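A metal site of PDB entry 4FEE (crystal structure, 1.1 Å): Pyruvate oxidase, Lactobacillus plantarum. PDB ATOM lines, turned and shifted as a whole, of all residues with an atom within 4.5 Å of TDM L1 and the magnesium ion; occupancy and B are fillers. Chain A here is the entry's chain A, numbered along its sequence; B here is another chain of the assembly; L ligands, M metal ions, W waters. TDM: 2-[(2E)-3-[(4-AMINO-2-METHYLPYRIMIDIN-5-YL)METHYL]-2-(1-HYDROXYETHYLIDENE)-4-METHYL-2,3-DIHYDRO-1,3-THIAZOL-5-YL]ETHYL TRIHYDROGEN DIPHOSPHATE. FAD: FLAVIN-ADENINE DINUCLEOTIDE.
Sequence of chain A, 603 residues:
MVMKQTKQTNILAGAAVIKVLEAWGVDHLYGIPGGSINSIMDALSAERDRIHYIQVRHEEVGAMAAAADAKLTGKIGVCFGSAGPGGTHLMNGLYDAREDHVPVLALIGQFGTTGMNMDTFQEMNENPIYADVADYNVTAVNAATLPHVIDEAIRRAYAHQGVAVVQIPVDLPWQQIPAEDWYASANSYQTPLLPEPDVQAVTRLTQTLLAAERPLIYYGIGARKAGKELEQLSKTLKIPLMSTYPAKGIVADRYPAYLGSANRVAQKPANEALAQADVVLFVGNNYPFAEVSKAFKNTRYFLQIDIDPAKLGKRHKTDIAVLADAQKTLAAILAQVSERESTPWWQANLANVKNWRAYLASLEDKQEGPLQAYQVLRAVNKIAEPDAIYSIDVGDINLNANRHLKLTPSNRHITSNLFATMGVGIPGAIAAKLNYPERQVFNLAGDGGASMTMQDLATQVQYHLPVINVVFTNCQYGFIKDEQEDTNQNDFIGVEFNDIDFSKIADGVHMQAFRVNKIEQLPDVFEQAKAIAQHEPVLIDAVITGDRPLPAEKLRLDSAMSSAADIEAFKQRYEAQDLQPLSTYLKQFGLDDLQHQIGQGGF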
ATOM      1  N   ASN A  92     -18.382 -32.043   4.751  1.00  0.00           N
ATOM      2  CA  ASN A  92     -18.478 -31.273   5.978  1.00  0.00           C
ATOM      3  C   ASN A  92     -17.096 -30.867   6.477  1.00  0.00           C
ATOM      4  O   ASN A  92     -16.939 -29.822   7.082  1.00  0.00           O
ATOM      5  CB  ASN A  92     -19.281 -31.981   7.069  1.00  0.00           C
ATOM      6  CG  ASN A  92     -20.754 -31.766   6.825  1.00  0.00           C
ATOM      7  OD1 ASN A  92     -21.240 -31.970   5.713  1.00  0.00           O
ATOM      8  ND2 ASN A  92     -21.489 -31.370   7.862  1.00  0.00           N
ATOM      9  N   VAL A 394     -19.816 -29.483  18.774  1.00  0.00           N
ATOM     10  CA  VAL A 394     -20.639 -28.289  18.533  1.00  0.00           C
ATOM     11  C   VAL A 394     -21.958 -28.439  19.254  1.00  0.00           C
ATOM     12  O   VAL A 394     -22.670 -29.441  19.033  1.00  0.00           O
ATOM     13  CB  VAL A 394     -20.836 -28.121  17.012  1.00  0.00           C
ATOM     14  CG1 VAL A 394     -21.898 -27.062  16.704  1.00  0.00           C
ATOM     15  CG2 VAL A 394     -19.534 -27.753  16.382  1.00  0.00           C
ATOM     16  N   GLY A 395     -22.326 -27.439  20.051  1.00  0.00           N
ATOM     17  CA  GLY A 395     -23.545 -27.450  20.800  1.00  0.00           C
ATOM     18  C   GLY A 395     -23.332 -26.785  22.158  1.00  0.00           C
ATOM     19  O   GLY A 395     -22.459 -25.925  22.317  1.00  0.00           O
ATOM     20  N   ASP A 396     -24.131 -27.184  23.155  1.00  0.00           N
ATOM     21  CA  ASP A 396     -23.915 -26.638  24.478  1.00  0.00           C
ATOM     22  C   ASP A 396     -22.486 -26.804  24.971  1.00  0.00           C
ATOM     23  O   ASP A 396     -22.025 -26.008  25.780  1.00  0.00           O
ATOM     24  CB  ASP A 396     -24.876 -27.263  25.490  1.00  0.00           C
ATOM     25  CG  ASP A 396     -26.256 -26.733  25.552  1.00  0.00           C
ATOM     26  OD1 ASP A 396     -26.554 -25.690  24.980  1.00  0.00           O
ATOM     27  OD2 ASP A 396     -27.082 -27.432  26.259  1.00  0.00           O
ATOM     28  N   ILE A 397     -21.751 -27.814  24.515  1.00  0.00           N
ATOM     29  CA  ILE A 397     -20.396 -27.992  24.969  1.00  0.00           C
ATOM     30  C   ILE A 397     -19.551 -26.779  24.653  1.00  0.00           C
ATOM     31  O   ILE A 397     -18.639 -26.470  25.435  1.00  0.00           O
ATOM     32  CB  ILE A 397     -19.734 -29.275  24.413  1.00  0.00           C
ATOM     33  CG1 ILE A 397     -18.397 -29.590  25.090  1.00  0.00           C
ATOM     34  CG2 ILE A 397     -19.582 -29.262  22.890  1.00  0.00           C
ATOM     35  CD1 ILE A 397     -18.442 -29.705  26.609  1.00  0.00           C
ATOM     36  N   ALA A 420     -19.333 -24.602  11.943  1.00  0.00           N
ATOM     37  CA  ALA A 420     -19.926 -25.232  13.093  1.00  0.00           C
ATOM     38  C   ALA A 420     -20.555 -26.567  12.740  1.00  0.00           C
ATOM     39  O   ALA A 420     -21.677 -26.873  13.154  1.00  0.00           O
ATOM     40  CB  ALA A 420     -20.896 -24.305  13.798  1.00  0.00           C
ATOM     41  N   THR A 421     -19.804 -27.419  12.051  1.00  0.00           N
ATOM     42  CA  THR A 421     -20.267 -28.798  11.850  1.00  0.00           C
ATOM     43  C   THR A 421     -20.148 -29.634  13.123  1.00  0.00           C
ATOM     44  O   THR A 421     -19.084 -29.785  13.681  1.00  0.00           O
ATOM     45  CB  THR A 421     -19.615 -29.467  10.659  1.00  0.00           C
ATOM     46  OG1 THR A 421     -20.200 -30.762  10.445  1.00  0.00           O
ATOM     47  CG2 THR A 421     -18.073 -29.608  10.797  1.00  0.00           C
ATOM     48  N   MET A 422     -21.291 -30.214  13.528  1.00  0.00           N
ATOM     49  CA  MET A 422     -21.243 -31.257  14.522  1.00  0.00           C
ATOM     50  C   MET A 422     -20.417 -32.429  14.011  1.00  0.00           C
ATOM     51  O   MET A 422     -20.260 -32.635  12.789  1.00  0.00           O
ATOM     52  CB  MET A 422     -22.679 -31.714  14.800  1.00  0.00           C
ATOM     53  CG  MET A 422     -23.549 -30.705  15.537  1.00  0.00           C
ATOM     54  SD  MET A 422     -25.261 -31.160  15.495  1.00  0.00           S
ATOM     55  CE  MET A 422     -25.264 -32.651  16.464  1.00  0.00           C
ATOM     56  N   GLY A 446     -21.145 -33.340  22.822  1.00  0.00           N
ATOM     57  CA  GLY A 446     -22.502 -33.699  23.118  1.00  0.00           C
ATOM     58  C   GLY A 446     -22.883 -35.031  22.489  1.00  0.00           C
ATOM     59  O   GLY A 446     -22.233 -35.525  21.562  1.00  0.00           O
ATOM     60  N   ASP A 447     -24.006 -35.571  22.954  1.00  0.00           N
ATOM     61  CA  ASP A 447     -24.483 -36.852  22.429  1.00  0.00           C
ATOM     62  C   ASP A 447     -24.898 -36.750  20.964  1.00  0.00           C
ATOM     63  O   ASP A 447     -24.646 -37.695  20.208  1.00  0.00           O
ATOM     64  CB  ASP A 447     -25.570 -37.451  23.316  1.00  0.00           C
ATOM     65  CG  ASP A 447     -26.744 -36.623  23.711  1.00  0.00           C
ATOM     66  OD1 ASP A 447     -26.819 -35.387  23.359  1.00  0.00           O
ATOM     67  OD2 ASP A 447     -27.644 -37.182  24.376  1.00  0.00           O
ATOM     68  N   GLY A 448     -25.495 -35.641  20.542  1.00  0.00           N
ATOM     69  CA  GLY A 448     -25.850 -35.503  19.147  1.00  0.00           C
ATOM     70  C   GLY A 448     -24.652 -35.523  18.242  1.00  0.00           C
ATOM     71  O   GLY A 448     -24.631 -36.204  17.218  1.00  0.00           O
ATOM     72  N   GLY A 449     -23.638 -34.748  18.608  1.00  0.00           N
ATOM     73  CA  GLY A 449     -22.427 -34.655  17.772  1.00  0.00           C
ATOM     74  C   GLY A 449     -21.595 -35.922  17.808  1.00  0.00           C
ATOM     75  O   GLY A 449     -21.108 -36.375  16.767  1.00  0.00           O
ATOM     76  N   MET A 452     -22.895 -38.519  15.493  1.00  0.00           N
ATOM     77  CA  MET A 452     -22.676 -38.374  14.057  1.00  0.00           C
ATOM     78  C   MET A 452     -21.388 -38.992  13.594  1.00  0.00           C
ATOM     79  O   MET A 452     -21.335 -39.393  12.426  1.00  0.00           O
ATOM     80  CB  MET A 452     -22.727 -36.890  13.679  1.00  0.00           C
ATOM     81  CG  MET A 452     -24.165 -36.395  13.657  1.00  0.00           C
ATOM     82  SD  MET A 452     -24.202 -34.657  13.192  1.00  0.00           S
ATOM     83  CE  MET A 452     -25.953 -34.382  13.250  1.00  0.00           C
ATOM     84  N   PHE A 472     -21.430 -35.852  26.606  1.00  0.00           N
ATOM     85  CA  PHE A 472     -22.419 -35.186  27.471  1.00  0.00           C
ATOM     86  C   PHE A 472     -23.808 -35.603  27.014  1.00  0.00           C
ATOM     87  O   PHE A 472     -24.350 -35.091  26.043  1.00  0.00           O
ATOM     88  CB  PHE A 472     -22.212 -33.665  27.406  1.00  0.00           C
ATOM     89  CG  PHE A 472     -20.923 -33.172  28.002  1.00  0.00           C
ATOM     90  CD1 PHE A 472     -19.664 -33.415  27.433  1.00  0.00           C
ATOM     91  CD2 PHE A 472     -20.954 -32.466  29.190  1.00  0.00           C
ATOM     92  CE1 PHE A 472     -18.530 -33.019  28.021  1.00  0.00           C
ATOM     93  CE2 PHE A 472     -19.779 -31.981  29.789  1.00  0.00           C
ATOM     94  CZ  PHE A 472     -18.548 -32.295  29.226  1.00  0.00           C
ATOM     95  N   ASN A 474     -27.460 -35.704  27.286  1.00  0.00           N
ATOM     96  CA  ASN A 474     -28.689 -35.118  27.750  1.00  0.00           C
ATOM     97  C   ASN A 474     -29.925 -35.667  27.018  1.00  0.00           C
ATOM     98  O   ASN A 474     -31.035 -35.247  27.347  1.00  0.00           O
ATOM     99  CB  ASN A 474     -28.646 -33.577  27.696  1.00  0.00           C
ATOM    100  CG  ASN A 474     -28.226 -33.014  26.394  1.00  0.00           C
ATOM    101  OD1 ASN A 474     -28.211 -33.704  25.361  1.00  0.00           O
ATOM    102  ND2 ASN A 474     -27.924 -31.716  26.367  1.00  0.00           N
ATOM    103  N   GLN A 476     -30.851 -34.858  24.145  1.00  0.00           N
ATOM    104  CA  GLN A 476     -31.385 -33.699  23.481  1.00  0.00           C
ATOM    105  C   GLN A 476     -30.391 -33.121  22.509  1.00  0.00           C
ATOM    106  O   GLN A 476     -29.144 -33.288  22.682  1.00  0.00           O
ATOM    107  CB  GLN A 476     -31.694 -32.586  24.466  1.00  0.00           C
ATOM    108  CG  GLN A 476     -32.656 -32.912  25.559  1.00  0.00           C
ATOM    109  CD  GLN A 476     -32.755 -31.770  26.563  1.00  0.00           C
ATOM    110  OE1 GLN A 476     -31.865 -30.948  26.678  1.00  0.00           O
ATOM    111  NE2 GLN A 476     -33.806 -31.733  27.304  1.00  0.00           N
ATOM    112  N   TYR A 477     -30.872 -32.371  21.543  1.00  0.00           N
ATOM    113  CA  TYR A 477     -30.090 -31.328  20.875  1.00  0.00           C
ATOM    114  C   TYR A 477     -30.305 -30.088  21.735  1.00  0.00           C
ATOM    115  O   TYR A 477     -31.177 -29.254  21.414  1.00  0.00           O
ATOM    116  CB  TYR A 477     -30.536 -31.113  19.437  1.00  0.00           C
ATOM    117  CG  TYR A 477     -30.316 -32.315  18.517  1.00  0.00           C
ATOM    118  CD1 TYR A 477     -29.093 -32.933  18.352  1.00  0.00           C
ATOM    119  CD2 TYR A 477     -31.361 -32.833  17.791  1.00  0.00           C
ATOM    120  CE1 TYR A 477     -28.933 -34.000  17.518  1.00  0.00           C
ATOM    121  CE2 TYR A 477     -31.202 -33.913  16.972  1.00  0.00           C
ATOM    122  CZ  TYR A 477     -30.014 -34.528  16.821  1.00  0.00           C
ATOM    123  OH  TYR A 477     -29.863 -35.604  15.992  1.00  0.00           O
ATOM    124  N   GLY A 478     -29.604 -30.000  22.847  1.00  0.00           N
ATOM    125  CA  GLY A 478     -29.938 -28.978  23.848  1.00  0.00           C
ATOM    126  C   GLY A 478     -29.820 -27.568  23.347  1.00  0.00           C
ATOM    127  O   GLY A 478     -30.698 -26.730  23.578  1.00  0.00           O
ATOM    128  N   PHE A 479     -28.763 -27.311  22.565  1.00  0.00           N
ATOM    129  CA  PHE A 479     -28.562 -25.975  22.046  1.00  0.00           C
ATOM    130  C   PHE A 479     -29.740 -25.546  21.194  1.00  0.00           C
ATOM    131  O   PHE A 479     -30.113 -24.370  21.214  1.00  0.00           O
ATOM    132  CB  PHE A 479     -27.250 -25.976  21.226  1.00  0.00           C
ATOM    133  CG  PHE A 479     -26.552 -24.659  20.992  1.00  0.00           C
ATOM    134  CD1 PHE A 479     -25.813 -24.058  22.026  1.00  0.00           C
ATOM    135  CD2 PHE A 479     -26.551 -24.057  19.749  1.00  0.00           C
ATOM    136  CE1 PHE A 479     -25.112 -22.875  21.824  1.00  0.00           C
ATOM    137  CE2 PHE A 479     -25.848 -22.888  19.548  1.00  0.00           C
ATOM    138  CZ  PHE A 479     -25.113 -22.316  20.584  1.00  0.00           C
ATOM    139  N   ILE A 480     -30.310 -26.467  20.433  1.00  0.00           N
ATOM    140  CA  ILE A 480     -31.466 -26.173  19.574  1.00  0.00           C
ATOM    141  C   ILE A 480     -32.777 -26.164  20.336  1.00  0.00           C
ATOM    142  O   ILE A 480     -33.666 -25.368  20.035  1.00  0.00           O
ATOM    143  CB  ILE A 480     -31.538 -27.150  18.416  1.00  0.00           C
ATOM    144  CG1 ILE A 480     -30.192 -27.226  17.704  1.00  0.00           C
ATOM    145  CG2 ILE A 480     -32.662 -26.841  17.440  1.00  0.00           C
ATOM    146  CD1 ILE A 480     -29.659 -25.890  17.299  1.00  0.00           C
ATOM    147  N   ILE B  32     -33.003 -33.002  10.859  1.00  0.00           N
ATOM    148  CA  ILE B  32     -32.506 -32.626  12.180  1.00  0.00           C
ATOM    149  C   ILE B  32     -32.700 -31.121  12.284  1.00  0.00           C
ATOM    150  O   ILE B  32     -32.368 -30.380  11.349  1.00  0.00           O
ATOM    151  CB  ILE B  32     -31.018 -32.984  12.357  1.00  0.00           C
ATOM    152  CG1 ILE B  32     -30.849 -34.514  12.387  1.00  0.00           C
ATOM    153  CG2 ILE B  32     -30.386 -32.318  13.573  1.00  0.00           C
ATOM    154  CD1 ILE B  32     -29.412 -34.998  12.445  1.00  0.00           C
ATOM    155  N   PRO B  33     -33.280 -30.630  13.380  1.00  0.00           N
ATOM    156  CA  PRO B  33     -33.596 -29.193  13.490  1.00  0.00           C
ATOM    157  C   PRO B  33     -32.336 -28.363  13.728  1.00  0.00           C
ATOM    158  O   PRO B  33     -31.277 -28.857  14.091  1.00  0.00           O
ATOM    159  CB  PRO B  33     -34.534 -29.117  14.684  1.00  0.00           C
ATOM    160  CG  PRO B  33     -34.042 -30.239  15.548  1.00  0.00           C
ATOM    161  CD  PRO B  33     -33.714 -31.354  14.574  1.00  0.00           C
ATOM    162  N   GLU B  59     -27.983 -36.290   9.063  1.00  0.00           N
ATOM    163  CA  GLU B  59     -28.827 -35.883   7.956  1.00  0.00           C
ATOM    164  C   GLU B  59     -28.628 -36.689   6.675  1.00  0.00           C
ATOM    165  O   GLU B  59     -29.552 -36.766   5.853  1.00  0.00           O
ATOM    166  CB  GLU B  59     -28.642 -34.395   7.641  1.00  0.00           C
ATOM    167  CG  GLU B  59     -28.946 -33.427   8.754  1.00  0.00           C
ATOM    168  CD  GLU B  59     -27.779 -33.143   9.692  1.00  0.00           C
ATOM    169  OE1 GLU B  59     -26.760 -33.867   9.705  1.00  0.00           O
ATOM    170  OE2 GLU B  59     -27.942 -32.168  10.488  1.00  0.00           O
ATOM    171  N   SER B  82     -30.334 -28.255   8.300  1.00  0.00           N
ATOM    172  CA  SER B  82     -30.053 -26.900   8.738  1.00  0.00           C
ATOM    173  C   SER B  82     -28.977 -26.247   7.896  1.00  0.00           C
ATOM    174  O   SER B  82     -28.260 -26.849   7.102  1.00  0.00           O
ATOM    175  CB  SER B  82     -29.712 -26.940  10.240  1.00  0.00           C
ATOM    176  OG  SER B  82     -28.544 -27.716  10.488  1.00  0.00           O
ATOM    177  N   PRO B  85     -23.735 -27.039   7.645  1.00  0.00           N
ATOM    178  CA  PRO B  85     -23.434 -28.472   7.787  1.00  0.00           C
ATOM    179  C   PRO B  85     -24.641 -29.394   7.786  1.00  0.00           C
ATOM    180  O   PRO B  85     -24.450 -30.597   7.478  1.00  0.00           O
ATOM    181  CB  PRO B  85     -22.685 -28.555   9.096  1.00  0.00           C
ATOM    182  CG  PRO B  85     -23.150 -27.337   9.878  1.00  0.00           C
ATOM    183  CD  PRO B  85     -23.233 -26.290   8.795  1.00  0.00           C
ATOM    184  N   GLY B  86     -25.823 -28.970   8.156  1.00  0.00           N
ATOM    185  CA  GLY B  86     -26.976 -29.870   8.072  1.00  0.00           C
ATOM    186  C   GLY B  86     -27.278 -30.243   6.630  1.00  0.00           C
ATOM    187  O   GLY B  86     -27.406 -31.403   6.295  1.00  0.00           O
ATOM    188  N   HIS B  89     -24.511 -32.362   4.828  1.00  0.00           N
ATOM    189  CA  HIS B  89     -24.650 -33.770   5.185  1.00  0.00           C
ATOM    190  C   HIS B  89     -25.654 -34.534   4.333  1.00  0.00           C
ATOM    191  O   HIS B  89     -25.593 -35.759   4.301  1.00  0.00           O
ATOM    192  CB  HIS B  89     -25.009 -33.925   6.647  1.00  0.00           C
ATOM    193  CG  HIS B  89     -23.885 -34.127   7.609  1.00  0.00           C
ATOM    194  ND1 HIS B  89     -24.097 -34.171   8.960  1.00  0.00           N
ATOM    195  CD2 HIS B  89     -22.573 -34.417   7.420  1.00  0.00           C
ATOM    196  CE1 HIS B  89     -22.961 -34.455   9.567  1.00  0.00           C
ATOM    197  NE2 HIS B  89     -22.004 -34.590   8.636  1.00  0.00           N
ATOM    198  N   PHE B 121     -22.753 -16.042  11.600  1.00  0.00           N
ATOM    199  CA  PHE B 121     -22.502 -17.387  12.022  1.00  0.00           C
ATOM    200  C   PHE B 121     -23.187 -18.391  11.109  1.00  0.00           C
ATOM    201  O   PHE B 121     -24.388 -18.293  10.893  1.00  0.00           O
ATOM    202  CB  PHE B 121     -23.002 -17.524  13.443  1.00  0.00           C
ATOM    203  CG  PHE B 121     -22.813 -18.935  14.030  1.00  0.00           C
ATOM    204  CD1 PHE B 121     -21.576 -19.386  14.395  1.00  0.00           C
ATOM    205  CD2 PHE B 121     -23.889 -19.773  14.156  1.00  0.00           C
ATOM    206  CE1 PHE B 121     -21.392 -20.648  14.897  1.00  0.00           C
ATOM    207  CE2 PHE B 121     -23.735 -21.049  14.711  1.00  0.00           C
ATOM    208  CZ  PHE B 121     -22.468 -21.481  15.067  1.00  0.00           C
ATOM    209  N   GLN B 122     -22.537 -19.425  10.591  1.00  0.00           N
ATOM    210  CA  GLN B 122     -23.070 -20.485   9.753  1.00  0.00           C
ATOM    211  C   GLN B 122     -23.706 -19.924   8.495  1.00  0.00           C
ATOM    212  O   GLN B 122     -24.487 -20.581   7.804  1.00  0.00           O
ATOM    213  CB  GLN B 122     -24.045 -21.440  10.450  1.00  0.00           C
ATOM    214  CG  GLN B 122     -23.284 -22.224  11.513  1.00  0.00           C
ATOM    215  CD  GLN B 122     -24.037 -23.395  12.037  1.00  0.00           C
ATOM    216  OE1 GLN B 122     -23.786 -24.574  11.763  1.00  0.00           O
ATOM    217  NE2 GLN B 122     -25.007 -23.067  12.828  1.00  0.00           N
HETATM  218  O1A TDM L   1     -26.424 -33.224  21.634  1.00  0.00           O
HETATM  219  PA  TDM L   1     -25.625 -32.132  20.981  1.00  0.00           P
HETATM  220  O2A TDM L   1     -24.358 -32.563  20.281  1.00  0.00           O
HETATM  221  O3A TDM L   1     -25.213 -31.040  22.049  1.00  0.00           O
HETATM  222  PB  TDM L   1     -26.053 -30.381  23.292  1.00  0.00           P
HETATM  223  O2B TDM L   1     -27.254 -31.275  23.523  1.00  0.00           O
HETATM  224  O3B TDM L   1     -26.398 -28.991  22.917  1.00  0.00           O
HETATM  225  O1B TDM L   1     -25.041 -30.483  24.424  1.00  0.00           O
HETATM  226  O7  TDM L   1     -26.605 -31.376  19.992  1.00  0.00           O
HETATM  227  C7  TDM L   1     -26.074 -30.300  19.095  1.00  0.00           C
HETATM  228  C6  TDM L   1     -27.318 -29.578  18.578  1.00  0.00           C
HETATM  229  C5  TDM L   1     -27.004 -28.616  17.449  1.00  0.00           C
HETATM  230  S1  TDM L   1     -25.976 -27.262  17.727  1.00  0.00           S
HETATM  231  C2  TDM L   1     -25.958 -26.827  16.005  1.00  0.00           C
HETATM  232  C27 TDM L   1     -25.834 -25.371  15.714  1.00  0.00           C
HETATM  233  C29 TDM L   1     -24.754 -24.721  16.577  1.00  0.00           C
HETATM  234  O28 TDM L   1     -25.490 -25.169  14.368  1.00  0.00           O
HETATM  235  N3  TDM L   1     -26.990 -27.636  15.375  1.00  0.00           N
HETATM  236  C4  TDM L   1     -27.476 -28.697  16.194  1.00  0.00           C
HETATM  237  CM4 TDM L   1     -28.451 -29.683  15.626  1.00  0.00           C
HETATM  238  C7' TDM L   1     -27.202 -27.590  13.946  1.00  0.00           C
HETATM  239  C5' TDM L   1     -26.379 -28.602  13.140  1.00  0.00           C
HETATM  240  C4' TDM L   1     -24.993 -28.536  13.016  1.00  0.00           C
HETATM  241  N4' TDM L   1     -24.327 -27.522  13.480  1.00  0.00           N
HETATM  242  N3' TDM L   1     -24.275 -29.532  12.337  1.00  0.00           N
HETATM  243  C2' TDM L   1     -25.030 -30.555  11.758  1.00  0.00           C
HETATM  244  CM2 TDM L   1     -24.236 -31.588  11.062  1.00  0.00           C
HETATM  245  N1' TDM L   1     -26.328 -30.586  11.783  1.00  0.00           N
HETATM  246  C6' TDM L   1     -27.068 -29.587  12.464  1.00  0.00           C
HETATM  247  PA  FAD L   2     -11.380 -15.589  12.802  1.00  0.00           P
HETATM  248  O1A FAD L   2     -10.574 -16.695  12.267  1.00  0.00           O
HETATM  249  O2A FAD L   2     -12.783 -15.420  12.286  1.00  0.00           O
HETATM  250  O5B FAD L   2     -10.673 -14.206  12.558  1.00  0.00           O
HETATM  251  C5B FAD L   2      -9.259 -14.028  12.855  1.00  0.00           C
HETATM  252  C4B FAD L   2      -8.945 -12.603  12.400  1.00  0.00           C
HETATM  253  O4B FAD L   2      -7.557 -12.357  12.701  1.00  0.00           O
HETATM  254  C3B FAD L   2      -9.107 -12.343  10.866  1.00  0.00           C
HETATM  255  O3B FAD L   2      -9.777 -11.089  10.629  1.00  0.00           O
HETATM  256  C2B FAD L   2      -7.678 -12.343  10.415  1.00  0.00           C
HETATM  257  O2B FAD L   2      -7.442 -11.596   9.195  1.00  0.00           O
HETATM  258  C1B FAD L   2      -6.887 -11.792  11.552  1.00  0.00           C
HETATM  259  N9A FAD L   2      -5.504 -12.058  11.633  1.00  0.00           N
HETATM  260  C8A FAD L   2      -4.934 -13.286  11.394  1.00  0.00           C
HETATM  261  N7A FAD L   2      -3.600 -13.255  11.683  1.00  0.00           N
HETATM  262  C5A FAD L   2      -3.365 -11.968  12.114  1.00  0.00           C
HETATM  263  C6A FAD L   2      -2.179 -11.345  12.567  1.00  0.00           C
HETATM  264  N6A FAD L   2      -0.964 -11.882  12.547  1.00  0.00           N
HETATM  265  N1A FAD L   2      -2.310 -10.039  12.977  1.00  0.00           N
HETATM  266  C2A FAD L   2      -3.496  -9.393  12.894  1.00  0.00           C
HETATM  267  N3A FAD L   2      -4.664  -9.936  12.468  1.00  0.00           N
HETATM  268  C4A FAD L   2      -4.533 -11.243  12.110  1.00  0.00           C
HETATM  269  N1  FAD L   2     -17.814 -16.883  19.107  1.00  0.00           N
HETATM  270  C2  FAD L   2     -18.098 -15.911  20.028  1.00  0.00           C
HETATM  271  O2  FAD L   2     -17.188 -15.130  20.383  1.00  0.00           O
HETATM  272  N3  FAD L   2     -19.353 -15.850  20.574  1.00  0.00           N
HETATM  273  C4  FAD L   2     -20.364 -16.716  20.288  1.00  0.00           C
HETATM  274  O4  FAD L   2     -21.493 -16.602  20.830  1.00  0.00           O
HETATM  275  C4X FAD L   2     -20.030 -17.812  19.409  1.00  0.00           C
HETATM  276  N5  FAD L   2     -21.016 -18.705  19.036  1.00  0.00           N
HETATM  277  C5X FAD L   2     -20.565 -19.938  18.580  1.00  0.00           C
HETATM  278  C6  FAD L   2     -21.387 -21.053  18.640  1.00  0.00           C
HETATM  279  C7  FAD L   2     -20.909 -22.312  18.228  1.00  0.00           C
HETATM  280  C7M FAD L   2     -21.828 -23.510  18.293  1.00  0.00           C
HETATM  281  C8  FAD L   2     -19.605 -22.401  17.725  1.00  0.00           C
HETATM  282  C8M FAD L   2     -19.041 -23.734  17.280  1.00  0.00           C
HETATM  283  C9  FAD L   2     -18.783 -21.274  17.649  1.00  0.00           C
HETATM  284  C9A FAD L   2     -19.258 -20.028  18.063  1.00  0.00           C
HETATM  285  N10 FAD L   2     -18.467 -18.857  17.985  1.00  0.00           N
HETATM  286  C10 FAD L   2     -18.774 -17.822  18.852  1.00  0.00           C
HETATM  287  C1' FAD L   2     -17.309 -18.728  17.112  1.00  0.00           C
HETATM  288  C2' FAD L   2     -17.630 -17.734  15.977  1.00  0.00           C
HETATM  289  O2' FAD L   2     -18.516 -18.363  15.020  1.00  0.00           O
HETATM  290  C3' FAD L   2     -16.416 -17.175  15.269  1.00  0.00           C
HETATM  291  O3' FAD L   2     -15.660 -18.266  14.707  1.00  0.00           O
HETATM  292  C4' FAD L   2     -15.466 -16.422  16.189  1.00  0.00           C
HETATM  293  O4' FAD L   2     -16.200 -15.475  17.036  1.00  0.00           O
HETATM  294  C5' FAD L   2     -14.476 -15.621  15.390  1.00  0.00           C
HETATM  295  O5' FAD L   2     -13.216 -15.647  16.124  1.00  0.00           O
HETATM  296  P   FAD L   2     -11.931 -14.899  15.616  1.00  0.00           P
HETATM  297  O1P FAD L   2     -12.254 -13.522  15.153  1.00  0.00           O
HETATM  298  O2P FAD L   2     -10.957 -15.097  16.732  1.00  0.00           O
HETATM  299  O3P FAD L   2     -11.402 -15.778  14.389  1.00  0.00           O
HETATM  300 MG    MG M   1     -27.254 -33.391  23.489  1.00  0.00          MG
HETATM  301  O   HOH W   1     -26.664 -25.854  11.047  1.00  0.00           O
HETATM  302  O   HOH W   2     -27.712 -22.708  16.485  1.00  0.00           O
HETATM  303  O   HOH W   3     -21.937 -31.575  20.700  1.00  0.00           O
HETATM  304  O   HOH W   4     -22.591 -30.173  23.208  1.00  0.00           O
HETATM  305  O   HOH W   5     -25.432 -33.195  24.543  1.00  0.00           O
HETATM  306  O   HOH W   6     -24.297 -30.535  27.063  1.00  0.00           O
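The backbone NH (N) of Asp 447 is in hydrogen-bond range of the backbone carbonyl oxygen (O) of Phe 472 (3.1 Å). The side-chain carboxylate of Glu 59 of chain B is in hydrogen-bond range of a ring nitrogen (ND1) of His 89 of chain B, 2.8 Å away. O of Ala 420 lies close to OE1 of Gln 122 of chain B. ND2 of Asn 92 sits close to NE2 of His 89 of chain B (3.4 Å). O of Pro 85 of chain B sits at hydrogen-bond distance from ND2 of Asn 92 (3.1 Å).
Within 4 Å of the magnesium ion: Asp 447, Asn 474 and Gln 476. The nearest printed residue that does not touch the magnesium ion is Gly 448 (4.1 Å).
A nitrogen (N1') of TDM L1 is in hydrogen-bond range of the side-chain carboxylate (OE2) of Glu 59 of chain B, at 2.6 Å. O28 of TDM L1 is in hydrogen-bond range of NE2 of Gln 122 of chain B (2.7 Å). O of Ala 420 sits at hydrogen-bond distance from N4' of TDM L1, 2.7 Å away. An oxygen (O3B) of TDM L1 lies within hydrogen-bond range of the backbone NH of Gly 478 (3.4 Å). The backbone NH (N) of Gly 448 sits at hydrogen-bond distance from an oxygen (O2A) of TDM L1 (3.3 Å). An oxygen (O2A) of TDM L1 is in hydrogen-bond range of the backbone NH (N) of Gly 449 (2.8 Å). The backbone NH (N) of Asp 396 lies within hydrogen-bond range of an oxygen (O3B) of TDM L1, at 2.9 Å. The backbone NH (N) of Phe 479 lies within hydrogen-bond range of an oxygen (O3B) of TDM L1 (2.9 Å). N3' of TDM L1 sits at hydrogen-bond distance from N of Met 422, at 3.3 Å.
Residues that only touch TDM L1: Ser 82 of chain B (3.1 Å), Pro 33 of chain B (3.3 Å), His 89 of chain B (3.3 Å), Tyr 477 (3.4 Å), Ile 480 (3.4 Å), Pro 85 of chain B (3.5 Å), Val 394 (3.5 Å), Gly 446 (3.6 Å), Met 452 (3.7 Å), Gly 86 of chain B (3.8 Å), Gly 395 (3.9 Å) and Ile 32 of chain B (3.9 Å). Hydrophobic or aromatic side chains within 4 Å of TDM L1: Val 394, Met 422, Met 452, Tyr 477, Phe 479, Ile 480, Ile 32 of chain B, Pro 85 of chain B and His 89 of chain B. Of the 29 residues printed, 24 come within 4 Å of TDM L1.
The magnesium ion is bound by an oxygen (O1A) of TDM L1 (2.0 Å). OD1 of Asp 447 binds the magnesium ion (2.0 Å). The magnesium ion is bound by the backbone carbonyl oxygen (O) of Gln 476, 2.1 Å away. Water W5 binds the magnesium ion, 2.1 Å away. The magnesium ion is bound by an oxygen (O2B) of TDM L1, at 2.1 Å. OD1 of Asn 474 is bound to the magnesium ion.
Water W5 lies within hydrogen-bond range of O of Phe 472 (2.6 Å), O1B of TDM L1 (2.7 Å), N of Asp 447 (3.2 Å) and ND2 of Asn 474 (3.4 Å). Water W3 lies within hydrogen-bond range of O2A of TDM L1 (2.6 Å), O of Val 394 (2.8 Å) and N of Gly 446 (2.9 Å). Water W4 lies within hydrogen-bond range of O1B of TDM L1 (2.8 Å), N of Ile 397 (2.8 Å) and N of Asp 396 (3.4 Å). Water W1 bridges the side-chain hydroxyl of Ser 82 of chain B (2.7 Å) and the side-chain amide oxygen of Gln 122 of chain B (3.2 Å).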
